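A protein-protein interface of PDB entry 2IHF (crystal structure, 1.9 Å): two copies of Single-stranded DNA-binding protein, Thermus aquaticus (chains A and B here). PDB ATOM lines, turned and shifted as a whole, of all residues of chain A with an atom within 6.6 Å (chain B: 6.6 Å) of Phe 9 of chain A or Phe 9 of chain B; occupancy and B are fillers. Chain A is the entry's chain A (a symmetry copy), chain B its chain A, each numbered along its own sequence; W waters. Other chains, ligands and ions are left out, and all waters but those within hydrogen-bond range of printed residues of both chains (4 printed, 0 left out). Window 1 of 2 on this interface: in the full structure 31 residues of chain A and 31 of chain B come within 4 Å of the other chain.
The backbone NH (N) of Phe 9 of chain A is in hydrogen-bond range of the backbone carbonyl oxygen (O) of Gln 130 of chain A (2.9 Å).
The backbone NH of Phe 9 of chain B lies within hydrogen-bond range of the backbone carbonyl oxygen of Gln 130 of chain B.
The backbone carbonyl oxygen (O) of Gln 7 of chain A lies within hydrogen-bond range of the backbone NH (N) of Ile 132 of chain A (2.9 Å).
The backbone NH (N) of Ile 132 of chain B lies within hydrogen-bond range of the backbone carbonyl oxygen (O) of Gln 7 of chain B.
OE1 of Gln 7 of chain B sits close to OE1 of Glu 79 of chain A, 2.7 Å away.
OE1 of Glu 79 of chain B sits close to OE1 of Gln 7 of chain A.
Of the 14 printed residues of chain B, 4 touch a printed residue of chain A.
Hydrophobic or aromatic side chains of chain B within 4 Å of the printed part of chain A: Phe 9 and Ile 132.
Along chain B the printed residues that touch a printed residue of chain A span positions 7 to 132.
Of the 14 printed residues of chain A, 4 touch a printed residue of chain B.
Hydrophobic or aromatic side chains of chain A within 4 Å of the printed part of chain B: Phe 9 and Ile 132.
Among the printed residues, 7 pairs touch across the chains.
Among the printed residues, no Asp or Glu carboxylate lies within 4 Å of a Lys or Arg side-chain nitrogen of the other chain.
Gln 7 of chain A touches Glu 79 of chain B, and with the chains exchanged Glu 79 of chain A touches Gln 7 of chain B.
Phe 9 of chain A touches its own counterpart, Phe 9 of chain B.
Phe 9 of chain A touches Ile 132 of chain B, and with the chains exchanged Ile 132 of chain A touches Phe 9 of chain B.
Glu 79 of chain A touches Ile 132 of chain B, and with the chains exchanged Ile 132 of chain A touches Glu 79 of chain B.
Of the 7 pairs that touch across the chains among the printed residues, 7 have their exchanged pair printed and touching as well.
Of the printed residues of chain B, Phe 9 of chain A touches Phe 9 (3.4 Å) and Ile 132 (3.4 Å).
Of the printed residues of chain A, Phe 9 of chain B touches Phe 9 (3.4 Å) and Ile 132 (3.4 Å).
Printed residues of chain A within 4 Å of Gln 7 of chain B: Glu 79 (2.7 Å).
Printed residues of chain B within 4 Å of Glu 79 of chain A: Gln 7 and Ile 132.
Printed residues of chain A within 4 Å of Ile 132 of chain B: Phe 9 (3.4 Å) and Glu 79 (3.5 Å).
Gly 80 of chain A touches none of the printed residues of chain B.
Ile 11 of chain A touches none of the printed residues of chain B.
The nearest printed residue of chain A that does not touch Phe 9 of chain B is Gln 7 of chain A (4.01 Å).
The nearest printed residue of chain B that does not touch Ile 132 of chain A is Phe 77 of chain B (4.4 Å).
Among the printed residues, pairs that only touch across the chains: Phe 9 of chain A with Phe 9 of chain B (3.4 Å), Phe 9 of chain A with Ile 132 of chain B (3.4 Å), Glu 79 of chain A with Ile 132 of chain B (3.5 Å), Ile 132 of chain A with Phe 9 of chain B (3.4 Å) and Ile 132 of chain A with Glu 79 of chain B (3.5 Å).
Water W2 lies within hydrogen-bond range of the side-chain amide oxygen (OE1) of Gln 130 of chain B (2.9 Å) and the side-chain amide oxygen (OE1) of Gln 130 of chain A (3.4 Å).
Water W1 bridges OE1 of Gln 130 of chain A and OE1 of Gln 130 of chain B.
Water W4 bridges OE1 of Gln 130 of chain B (3.0 Å) and OE1 of Gln 130 of chain A (3.1 Å).
Water W3 bridges OE1 of Gln 130 of chain A (3.0 Å) and OE1 of Gln 130 of chain B (3.1 Å).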
ATOM      1  N   GLN A   7     -25.233 -14.330  28.462  1.00  0.00           N
ATOM      2  CA  GLN A   7     -25.112 -13.068  27.742  1.00  0.00           C
ATOM      3  C   GLN A   7     -26.348 -12.779  26.908  1.00  0.00           C
ATOM      4  O   GLN A   7     -26.891 -13.679  26.266  1.00  0.00           O
ATOM      5  CB  GLN A   7     -23.881 -13.109  26.849  1.00  0.00           C
ATOM      6  CG  GLN A   7     -22.638 -13.588  27.573  1.00  0.00           C
ATOM      7  CD  GLN A   7     -21.532 -13.990  26.623  1.00  0.00           C
ATOM      8  OE1 GLN A   7     -21.776 -14.698  25.643  1.00  0.00           O
ATOM      9  NE2 GLN A   7     -20.307 -13.554  26.909  1.00  0.00           N
ATOM     10  N   VAL A   8     -26.787 -11.519  26.938  1.00  0.00           N
ATOM     11  CA  VAL A   8     -27.966 -11.073  26.198  1.00  0.00           C
ATOM     12  C   VAL A   8     -27.627  -9.837  25.365  1.00  0.00           C
ATOM     13  O   VAL A   8     -26.945  -8.929  25.839  1.00  0.00           O
ATOM     14  CB  VAL A   8     -29.146 -10.729  27.155  1.00  0.00           C
ATOM     15  CG1 VAL A   8     -30.364 -10.301  26.363  1.00  0.00           C
ATOM     16  CG2 VAL A   8     -29.497 -11.925  28.004  1.00  0.00           C
ATOM     17  N   PHE A   9     -28.091  -9.822  24.116  1.00  0.00           N
ATOM     18  CA  PHE A   9     -27.859  -8.706  23.201  1.00  0.00           C
ATOM     19  C   PHE A   9     -29.209  -8.338  22.621  1.00  0.00           C
ATOM     20  O   PHE A   9     -29.883  -9.186  22.036  1.00  0.00           O
ATOM     21  CB  PHE A   9     -26.930  -9.107  22.048  1.00  0.00           C
ATOM     22  CG  PHE A   9     -25.732  -9.917  22.479  1.00  0.00           C
ATOM     23  CD1 PHE A   9     -25.868 -11.279  22.790  1.00  0.00           C
ATOM     24  CD2 PHE A   9     -24.470  -9.321  22.577  1.00  0.00           C
ATOM     25  CE1 PHE A   9     -24.766 -12.037  23.189  1.00  0.00           C
ATOM     26  CE2 PHE A   9     -23.364 -10.066  22.974  1.00  0.00           C
ATOM     27  CZ  PHE A   9     -23.510 -11.430  23.280  1.00  0.00           C
ATOM     28  N   LEU A  10     -29.598  -7.081  22.778  1.00  0.00           N
ATOM     29  CA  LEU A  10     -30.871  -6.624  22.266  1.00  0.00           C
ATOM     30  C   LEU A  10     -30.769  -5.256  21.635  1.00  0.00           C
ATOM     31  O   LEU A  10     -29.926  -4.446  22.007  1.00  0.00           O
ATOM     32  CB  LEU A  10     -31.907  -6.511  23.397  1.00  0.00           C
ATOM     33  CG  LEU A  10     -32.392  -7.731  24.185  1.00  0.00           C
ATOM     34  CD1 LEU A  10     -33.146  -7.270  25.432  1.00  0.00           C
ATOM     35  CD2 LEU A  10     -33.274  -8.610  23.301  1.00  0.00           C
ATOM     36  N   ILE A  11     -31.638  -5.023  20.660  1.00  0.00           N
ATOM     37  CA  ILE A  11     -31.805  -3.722  20.023  1.00  0.00           C
ATOM     38  C   ILE A  11     -33.320  -3.676  19.880  1.00  0.00           C
ATOM     39  O   ILE A  11     -33.915  -4.515  19.210  1.00  0.00           O
ATOM     40  CB  ILE A  11     -31.165  -3.595  18.636  1.00  0.00           C
ATOM     41  CG1 ILE A  11     -29.637  -3.602  18.757  1.00  0.00           C
ATOM     42  CG2 ILE A  11     -31.626  -2.286  17.990  1.00  0.00           C
ATOM     43  CD1 ILE A  11     -28.913  -3.458  17.446  1.00  0.00           C
ATOM     44  N   PHE A  77     -29.614  -0.065  22.096  1.00  0.00           N
ATOM     45  CA  PHE A  77     -28.823  -1.287  21.991  1.00  0.00           C
ATOM     46  C   PHE A  77     -28.536  -1.664  23.434  1.00  0.00           C
ATOM     47  O   PHE A  77     -28.153  -0.811  24.238  1.00  0.00           O
ATOM     48  CB  PHE A  77     -27.494  -1.051  21.272  1.00  0.00           C
ATOM     49  CG  PHE A  77     -26.501  -2.169  21.448  1.00  0.00           C
ATOM     50  CD1 PHE A  77     -26.857  -3.488  21.171  1.00  0.00           C
ATOM     51  CD2 PHE A  77     -25.202  -1.902  21.868  1.00  0.00           C
ATOM     52  CE1 PHE A  77     -25.935  -4.526  21.299  1.00  0.00           C
ATOM     53  CE2 PHE A  77     -24.272  -2.936  22.000  1.00  0.00           C
ATOM     54  CZ  PHE A  77     -24.641  -4.250  21.715  1.00  0.00           C
ATOM     55  N   VAL A  78     -28.727  -2.936  23.763  1.00  0.00           N
ATOM     56  CA  VAL A  78     -28.494  -3.417  25.115  1.00  0.00           C
ATOM     57  C   VAL A  78     -27.602  -4.652  25.168  1.00  0.00           C
ATOM     58  O   VAL A  78     -27.669  -5.517  24.307  1.00  0.00           O
ATOM     59  CB  VAL A  78     -29.830  -3.802  25.828  1.00  0.00           C
ATOM     60  CG1 VAL A  78     -29.541  -4.346  27.215  1.00  0.00           C
ATOM     61  CG2 VAL A  78     -30.753  -2.609  25.921  1.00  0.00           C
ATOM     62  N   GLU A  79     -26.751  -4.700  26.184  1.00  0.00           N
ATOM     63  CA  GLU A  79     -25.924  -5.864  26.433  1.00  0.00           C
ATOM     64  C   GLU A  79     -25.983  -6.066  27.920  1.00  0.00           C
ATOM     65  O   GLU A  79     -25.742  -5.142  28.691  1.00  0.00           O
ATOM     66  CB  GLU A  79     -24.483  -5.672  25.985  1.00  0.00           C
ATOM     67  CG  GLU A  79     -24.285  -6.102  24.551  1.00  0.00           C
ATOM     68  CD  GLU A  79     -22.870  -6.547  24.243  1.00  0.00           C
ATOM     69  OE1 GLU A  79     -22.633  -6.950  23.078  1.00  0.00           O
ATOM     70  OE2 GLU A  79     -22.008  -6.495  25.157  1.00  0.00           O
ATOM     71  N   GLY A  80     -26.351  -7.274  28.313  1.00  0.00           N
ATOM     72  CA  GLY A  80     -26.445  -7.596  29.716  1.00  0.00           C
ATOM     73  C   GLY A  80     -26.521  -9.095  29.901  1.00  0.00           C
ATOM     74  O   GLY A  80     -25.948  -9.863  29.128  1.00  0.00           O
ATOM     75  N   LEU A 128     -32.991  -6.617  17.334  1.00  0.00           N
ATOM     76  CA  LEU A 128     -32.062  -7.718  17.531  1.00  0.00           C
ATOM     77  C   LEU A 128     -32.431  -8.410  18.843  1.00  0.00           C
ATOM     78  O   LEU A 128     -32.762  -7.747  19.834  1.00  0.00           O
ATOM     79  CB  LEU A 128     -30.636  -7.174  17.619  1.00  0.00           C
ATOM     80  CG  LEU A 128     -29.535  -8.186  17.915  1.00  0.00           C
ATOM     81  CD1 LEU A 128     -29.215  -8.936  16.642  1.00  0.00           C
ATOM     82  CD2 LEU A 128     -28.304  -7.477  18.426  1.00  0.00           C
ATOM     83  N   ASN A 129     -32.359  -9.736  18.855  1.00  0.00           N
ATOM     84  CA  ASN A 129     -32.703 -10.506  20.048  1.00  0.00           C
ATOM     85  C   ASN A 129     -31.864 -11.778  20.067  1.00  0.00           C
ATOM     86  O   ASN A 129     -32.208 -12.747  19.403  1.00  0.00           O
ATOM     87  CB  ASN A 129     -34.199 -10.849  20.020  1.00  0.00           C
ATOM     88  CG  ASN A 129     -34.662 -11.580  21.265  1.00  0.00           C
ATOM     89  OD1 ASN A 129     -33.863 -11.925  22.131  1.00  0.00           O
ATOM     90  ND2 ASN A 129     -35.960 -11.827  21.353  1.00  0.00           N
ATOM     91  N   GLN A 130     -30.759 -11.771  20.811  1.00  0.00           N
ATOM     92  CA  GLN A 130     -29.891 -12.949  20.880  1.00  0.00           C
ATOM     93  C   GLN A 130     -29.422 -13.243  22.301  1.00  0.00           C
ATOM     94  O   GLN A 130     -29.055 -12.335  23.040  1.00  0.00           O
ATOM     95  CB  GLN A 130     -28.652 -12.770  19.992  1.00  0.00           C
ATOM     96  CG  GLN A 130     -28.937 -12.280  18.579  1.00  0.00           C
ATOM     97  CD  GLN A 130     -27.672 -12.044  17.767  1.00  0.00           C
ATOM     98  OE1 GLN A 130     -26.621 -11.715  18.318  1.00  0.00           O
ATOM     99  NE2 GLN A 130     -27.774 -12.195  16.450  1.00  0.00           N
ATOM    100  N   VAL A 131     -29.421 -14.519  22.672  1.00  0.00           N
ATOM    101  CA  VAL A 131     -28.976 -14.943  23.993  1.00  0.00           C
ATOM    102  C   VAL A 131     -27.988 -16.095  23.826  1.00  0.00           C
ATOM    103  O   VAL A 131     -28.166 -16.940  22.949  1.00  0.00           O
ATOM    104  CB  VAL A 131     -30.161 -15.459  24.871  1.00  0.00           C
ATOM    105  CG1 VAL A 131     -29.664 -15.855  26.255  1.00  0.00           C
ATOM    106  CG2 VAL A 131     -31.229 -14.397  25.002  1.00  0.00           C
ATOM    107  N   ILE A 132     -26.931 -16.108  24.641  1.00  0.00           N
ATOM    108  CA  ILE A 132     -25.975 -17.211  24.629  1.00  0.00           C
ATOM    109  C   ILE A 132     -25.923 -17.713  26.058  1.00  0.00           C
ATOM    110  O   ILE A 132     -25.614 -16.958  26.974  1.00  0.00           O
ATOM    111  CB  ILE A 132     -24.548 -16.803  24.254  1.00  0.00           C
ATOM    112  CG1 ILE A 132     -24.496 -16.219  22.844  1.00  0.00           C
ATOM    113  CG2 ILE A 132     -23.651 -18.025  24.316  1.00  0.00           C
ATOM    114  CD1 ILE A 132     -23.078 -15.924  22.366  1.00  0.00           C
ATOM    115  N   GLN B   7     -16.182  -7.831  20.408  1.00  0.00           N
ATOM    116  CA  GLN B   7     -16.525  -9.194  20.798  1.00  0.00           C
ATOM    117  C   GLN B   7     -16.661 -10.103  19.589  1.00  0.00           C
ATOM    118  O   GLN B   7     -17.232  -9.708  18.572  1.00  0.00           O
ATOM    119  CB  GLN B   7     -17.826  -9.183  21.589  1.00  0.00           C
ATOM    120  CG  GLN B   7     -17.838  -8.147  22.696  1.00  0.00           C
ATOM    121  CD  GLN B   7     -19.231  -7.876  23.218  1.00  0.00           C
ATOM    122  OE1 GLN B   7     -20.169  -7.703  22.438  1.00  0.00           O
ATOM    123  NE2 GLN B   7     -19.376  -7.822  24.542  1.00  0.00           N
ATOM    124  N   VAL B   8     -16.119 -11.317  19.712  1.00  0.00           N
ATOM    125  CA  VAL B   8     -16.155 -12.313  18.643  1.00  0.00           C
ATOM    126  C   VAL B   8     -16.694 -13.638  19.179  1.00  0.00           C
ATOM    127  O   VAL B   8     -16.325 -14.071  20.270  1.00  0.00           O
ATOM    128  CB  VAL B   8     -14.741 -12.551  18.035  1.00  0.00           C
ATOM    129  CG1 VAL B   8     -14.811 -13.561  16.910  1.00  0.00           C
ATOM    130  CG2 VAL B   8     -14.173 -11.256  17.510  1.00  0.00           C
ATOM    131  N   PHE B   9     -17.584 -14.266  18.411  1.00  0.00           N
ATOM    132  CA  PHE B   9     -18.181 -15.548  18.782  1.00  0.00           C
ATOM    133  C   PHE B   9     -18.028 -16.458  17.581  1.00  0.00           C
ATOM    134  O   PHE B   9     -18.481 -16.121  16.487  1.00  0.00           O
ATOM    135  CB  PHE B   9     -19.677 -15.404  19.091  1.00  0.00           C
ATOM    136  CG  PHE B   9     -20.014 -14.205  19.942  1.00  0.00           C
ATOM    137  CD1 PHE B   9     -20.047 -12.919  19.380  1.00  0.00           C
ATOM    138  CD2 PHE B   9     -20.296 -14.357  21.304  1.00  0.00           C
ATOM    139  CE1 PHE B   9     -20.359 -11.803  20.158  1.00  0.00           C
ATOM    140  CE2 PHE B   9     -20.608 -13.252  22.091  1.00  0.00           C
ATOM    141  CZ  PHE B   9     -20.640 -11.969  21.517  1.00  0.00           C
ATOM    142  N   LEU B  10     -17.397 -17.606  17.784  1.00  0.00           N
ATOM    143  CA  LEU B  10     -17.192 -18.547  16.705  1.00  0.00           C
ATOM    144  C   LEU B  10     -17.422 -19.972  17.146  1.00  0.00           C
ATOM    145  O   LEU B  10     -17.235 -20.315  18.309  1.00  0.00           O
ATOM    146  CB  LEU B  10     -15.748 -18.474  16.182  1.00  0.00           C
ATOM    147  CG  LEU B  10     -15.184 -17.218  15.513  1.00  0.00           C
ATOM    148  CD1 LEU B  10     -13.663 -17.333  15.407  1.00  0.00           C
ATOM    149  CD2 LEU B  10     -15.819 -17.027  14.138  1.00  0.00           C
ATOM    150  N   ILE B  11     -17.849 -20.790  16.193  1.00  0.00           N
ATOM    151  CA  ILE B  11     -17.989 -22.232  16.371  1.00  0.00           C
ATOM    152  C   ILE B  11     -17.472 -22.728  15.029  1.00  0.00           C
ATOM    153  O   ILE B  11     -18.029 -22.412  13.982  1.00  0.00           O
ATOM    154  CB  ILE B  11     -19.428 -22.720  16.568  1.00  0.00           C
ATOM    155  CG1 ILE B  11     -19.960 -22.262  17.932  1.00  0.00           C
ATOM    156  CG2 ILE B  11     -19.453 -24.249  16.492  1.00  0.00           C
ATOM    157  CD1 ILE B  11     -21.364 -22.713  18.230  1.00  0.00           C
ATOM    158  N   PHE B  77     -16.128 -24.055  20.332  1.00  0.00           N
ATOM    159  CA  PHE B  77     -16.872 -22.811  20.508  1.00  0.00           C
ATOM    160  C   PHE B  77     -15.835 -21.834  21.036  1.00  0.00           C
ATOM    161  O   PHE B  77     -15.068 -22.167  21.944  1.00  0.00           O
ATOM    162  CB  PHE B  77     -17.986 -22.951  21.545  1.00  0.00           C
ATOM    163  CG  PHE B  77     -18.542 -21.634  22.021  1.00  0.00           C
ATOM    164  CD1 PHE B  77     -18.985 -20.676  21.109  1.00  0.00           C
ATOM    165  CD2 PHE B  77     -18.646 -21.359  23.380  1.00  0.00           C
ATOM    166  CE1 PHE B  77     -19.530 -19.468  21.541  1.00  0.00           C
ATOM    167  CE2 PHE B  77     -19.191 -20.152  23.822  1.00  0.00           C
ATOM    168  CZ  PHE B  77     -19.633 -19.205  22.899  1.00  0.00           C
ATOM    169  N   VAL B  78     -15.806 -20.635  20.466  1.00  0.00           N
ATOM    170  CA  VAL B  78     -14.853 -19.618  20.879  1.00  0.00           C
ATOM    171  C   VAL B  78     -15.504 -18.274  21.185  1.00  0.00           C
ATOM    172  O   VAL B  78     -16.455 -17.870  20.531  1.00  0.00           O
ATOM    173  CB  VAL B  78     -13.779 -19.351  19.776  1.00  0.00           C
ATOM    174  CG1 VAL B  78     -12.836 -18.250  20.224  1.00  0.00           C
ATOM    175  CG2 VAL B  78     -12.999 -20.609  19.471  1.00  0.00           C
ATOM    176  N   GLU B  79     -14.987 -17.606  22.207  1.00  0.00           N
ATOM    177  CA  GLU B  79     -15.421 -16.265  22.542  1.00  0.00           C
ATOM    178  C   GLU B  79     -14.156 -15.517  22.850  1.00  0.00           C
ATOM    179  O   GLU B  79     -13.341 -15.963  23.652  1.00  0.00           O
ATOM    180  CB  GLU B  79     -16.360 -16.229  23.739  1.00  0.00           C
ATOM    181  CG  GLU B  79     -17.803 -16.364  23.318  1.00  0.00           C
ATOM    182  CD  GLU B  79     -18.777 -15.719  24.283  1.00  0.00           C
ATOM    183  OE1 GLU B  79     -19.996 -15.759  23.986  1.00  0.00           O
ATOM    184  OE2 GLU B  79     -18.327 -15.176  25.324  1.00  0.00           O
ATOM    185  N   GLY B  80     -13.981 -14.396  22.171  1.00  0.00           N
ATOM    186  CA  GLY B  80     -12.807 -13.584  22.377  1.00  0.00           C
ATOM    187  C   GLY B  80     -13.011 -12.212  21.776  1.00  0.00           C
ATOM    188  O   GLY B  80     -14.124 -11.689  21.743  1.00  0.00           O
ATOM    189  N   LEU B 128     -20.602 -21.056  13.404  1.00  0.00           N
ATOM    190  CA  LEU B 128     -21.107 -19.764  13.837  1.00  0.00           C
ATOM    191  C   LEU B 128     -19.996 -18.735  13.631  1.00  0.00           C
ATOM    192  O   LEU B 128     -18.821 -19.016  13.897  1.00  0.00           O
ATOM    193  CB  LEU B 128     -21.480 -19.829  15.318  1.00  0.00           C
ATOM    194  CG  LEU B 128     -21.948 -18.532  15.965  1.00  0.00           C
ATOM    195  CD1 LEU B 128     -23.387 -18.288  15.571  1.00  0.00           C
ATOM    196  CD2 LEU B 128     -21.826 -18.629  17.467  1.00  0.00           C
ATOM    197  N   ASN B 129     -20.366 -17.545  13.175  1.00  0.00           N
ATOM    198  CA  ASN B 129     -19.389 -16.487  12.925  1.00  0.00           C
ATOM    199  C   ASN B 129     -20.057 -15.138  13.160  1.00  0.00           C
ATOM    200  O   ASN B 129     -20.748 -14.638  12.282  1.00  0.00           O
ATOM    201  CB  ASN B 129     -18.881 -16.593  11.480  1.00  0.00           C
ATOM    202  CG  ASN B 129     -17.799 -15.582  11.157  1.00  0.00           C
ATOM    203  OD1 ASN B 129     -17.470 -14.725  11.972  1.00  0.00           O
ATOM    204  ND2 ASN B 129     -17.249 -15.673   9.956  1.00  0.00           N
ATOM    205  N   GLN B 130     -19.868 -14.559  14.344  1.00  0.00           N
ATOM    206  CA  GLN B 130     -20.480 -13.266  14.656  1.00  0.00           C
ATOM    207  C   GLN B 130     -19.515 -12.323  15.369  1.00  0.00           C
ATOM    208  O   GLN B 130     -18.785 -12.734  16.265  1.00  0.00           O
ATOM    209  CB  GLN B 130     -21.720 -13.446  15.542  1.00  0.00           C
ATOM    210  CG  GLN B 130     -22.702 -14.508  15.069  1.00  0.00           C
ATOM    211  CD  GLN B 130     -23.871 -14.702  16.022  1.00  0.00           C
ATOM    212  OE1 GLN B 130     -23.741 -14.497  17.229  1.00  0.00           O
ATOM    213  NE2 GLN B 130     -25.015 -15.115  15.485  1.00  0.00           N
ATOM    214  N   VAL B 131     -19.531 -11.054  14.976  1.00  0.00           N
ATOM    215  CA  VAL B 131     -18.678 -10.042  15.588  1.00  0.00           C
ATOM    216  C   VAL B 131     -19.539  -8.832  15.944  1.00  0.00           C
ATOM    217  O   VAL B 131     -20.452  -8.481  15.197  1.00  0.00           O
ATOM    218  CB  VAL B 131     -17.558  -9.556  14.612  1.00  0.00           C
ATOM    219  CG1 VAL B 131     -16.666  -8.530  15.299  1.00  0.00           C
ATOM    220  CG2 VAL B 131     -16.719 -10.722  14.140  1.00  0.00           C
ATOM    221  N   ILE B 132     -19.272  -8.220  17.099  1.00  0.00           N
ATOM    222  CA  ILE B 132     -19.973  -7.001  17.493  1.00  0.00           C
ATOM    223  C   ILE B 132     -18.883  -5.983  17.764  1.00  0.00           C
ATOM    224  O   ILE B 132     -18.015  -6.205  18.601  1.00  0.00           O
ATOM    225  CB  ILE B 132     -20.784  -7.130  18.785  1.00  0.00           C
ATOM    226  CG1 ILE B 132     -21.878  -8.186  18.644  1.00  0.00           C
ATOM    227  CG2 ILE B 132     -21.425  -5.793  19.103  1.00  0.00           C
ATOM    228  CD1 ILE B 132     -22.805  -8.258  19.852  1.00  0.00           C
HETATM  229  O   HOH W   1     -23.731 -11.332  18.409  1.00  0.00           O
HETATM  230  O   HOH W   2     -24.762 -14.033  19.923  1.00  0.00           O
HETATM  231  O   HOH W   3     -24.679 -11.769  16.009  1.00  0.00           O
HETATM  232  O   HOH W   4     -26.573 -14.845  18.215  1.00  0.00           O
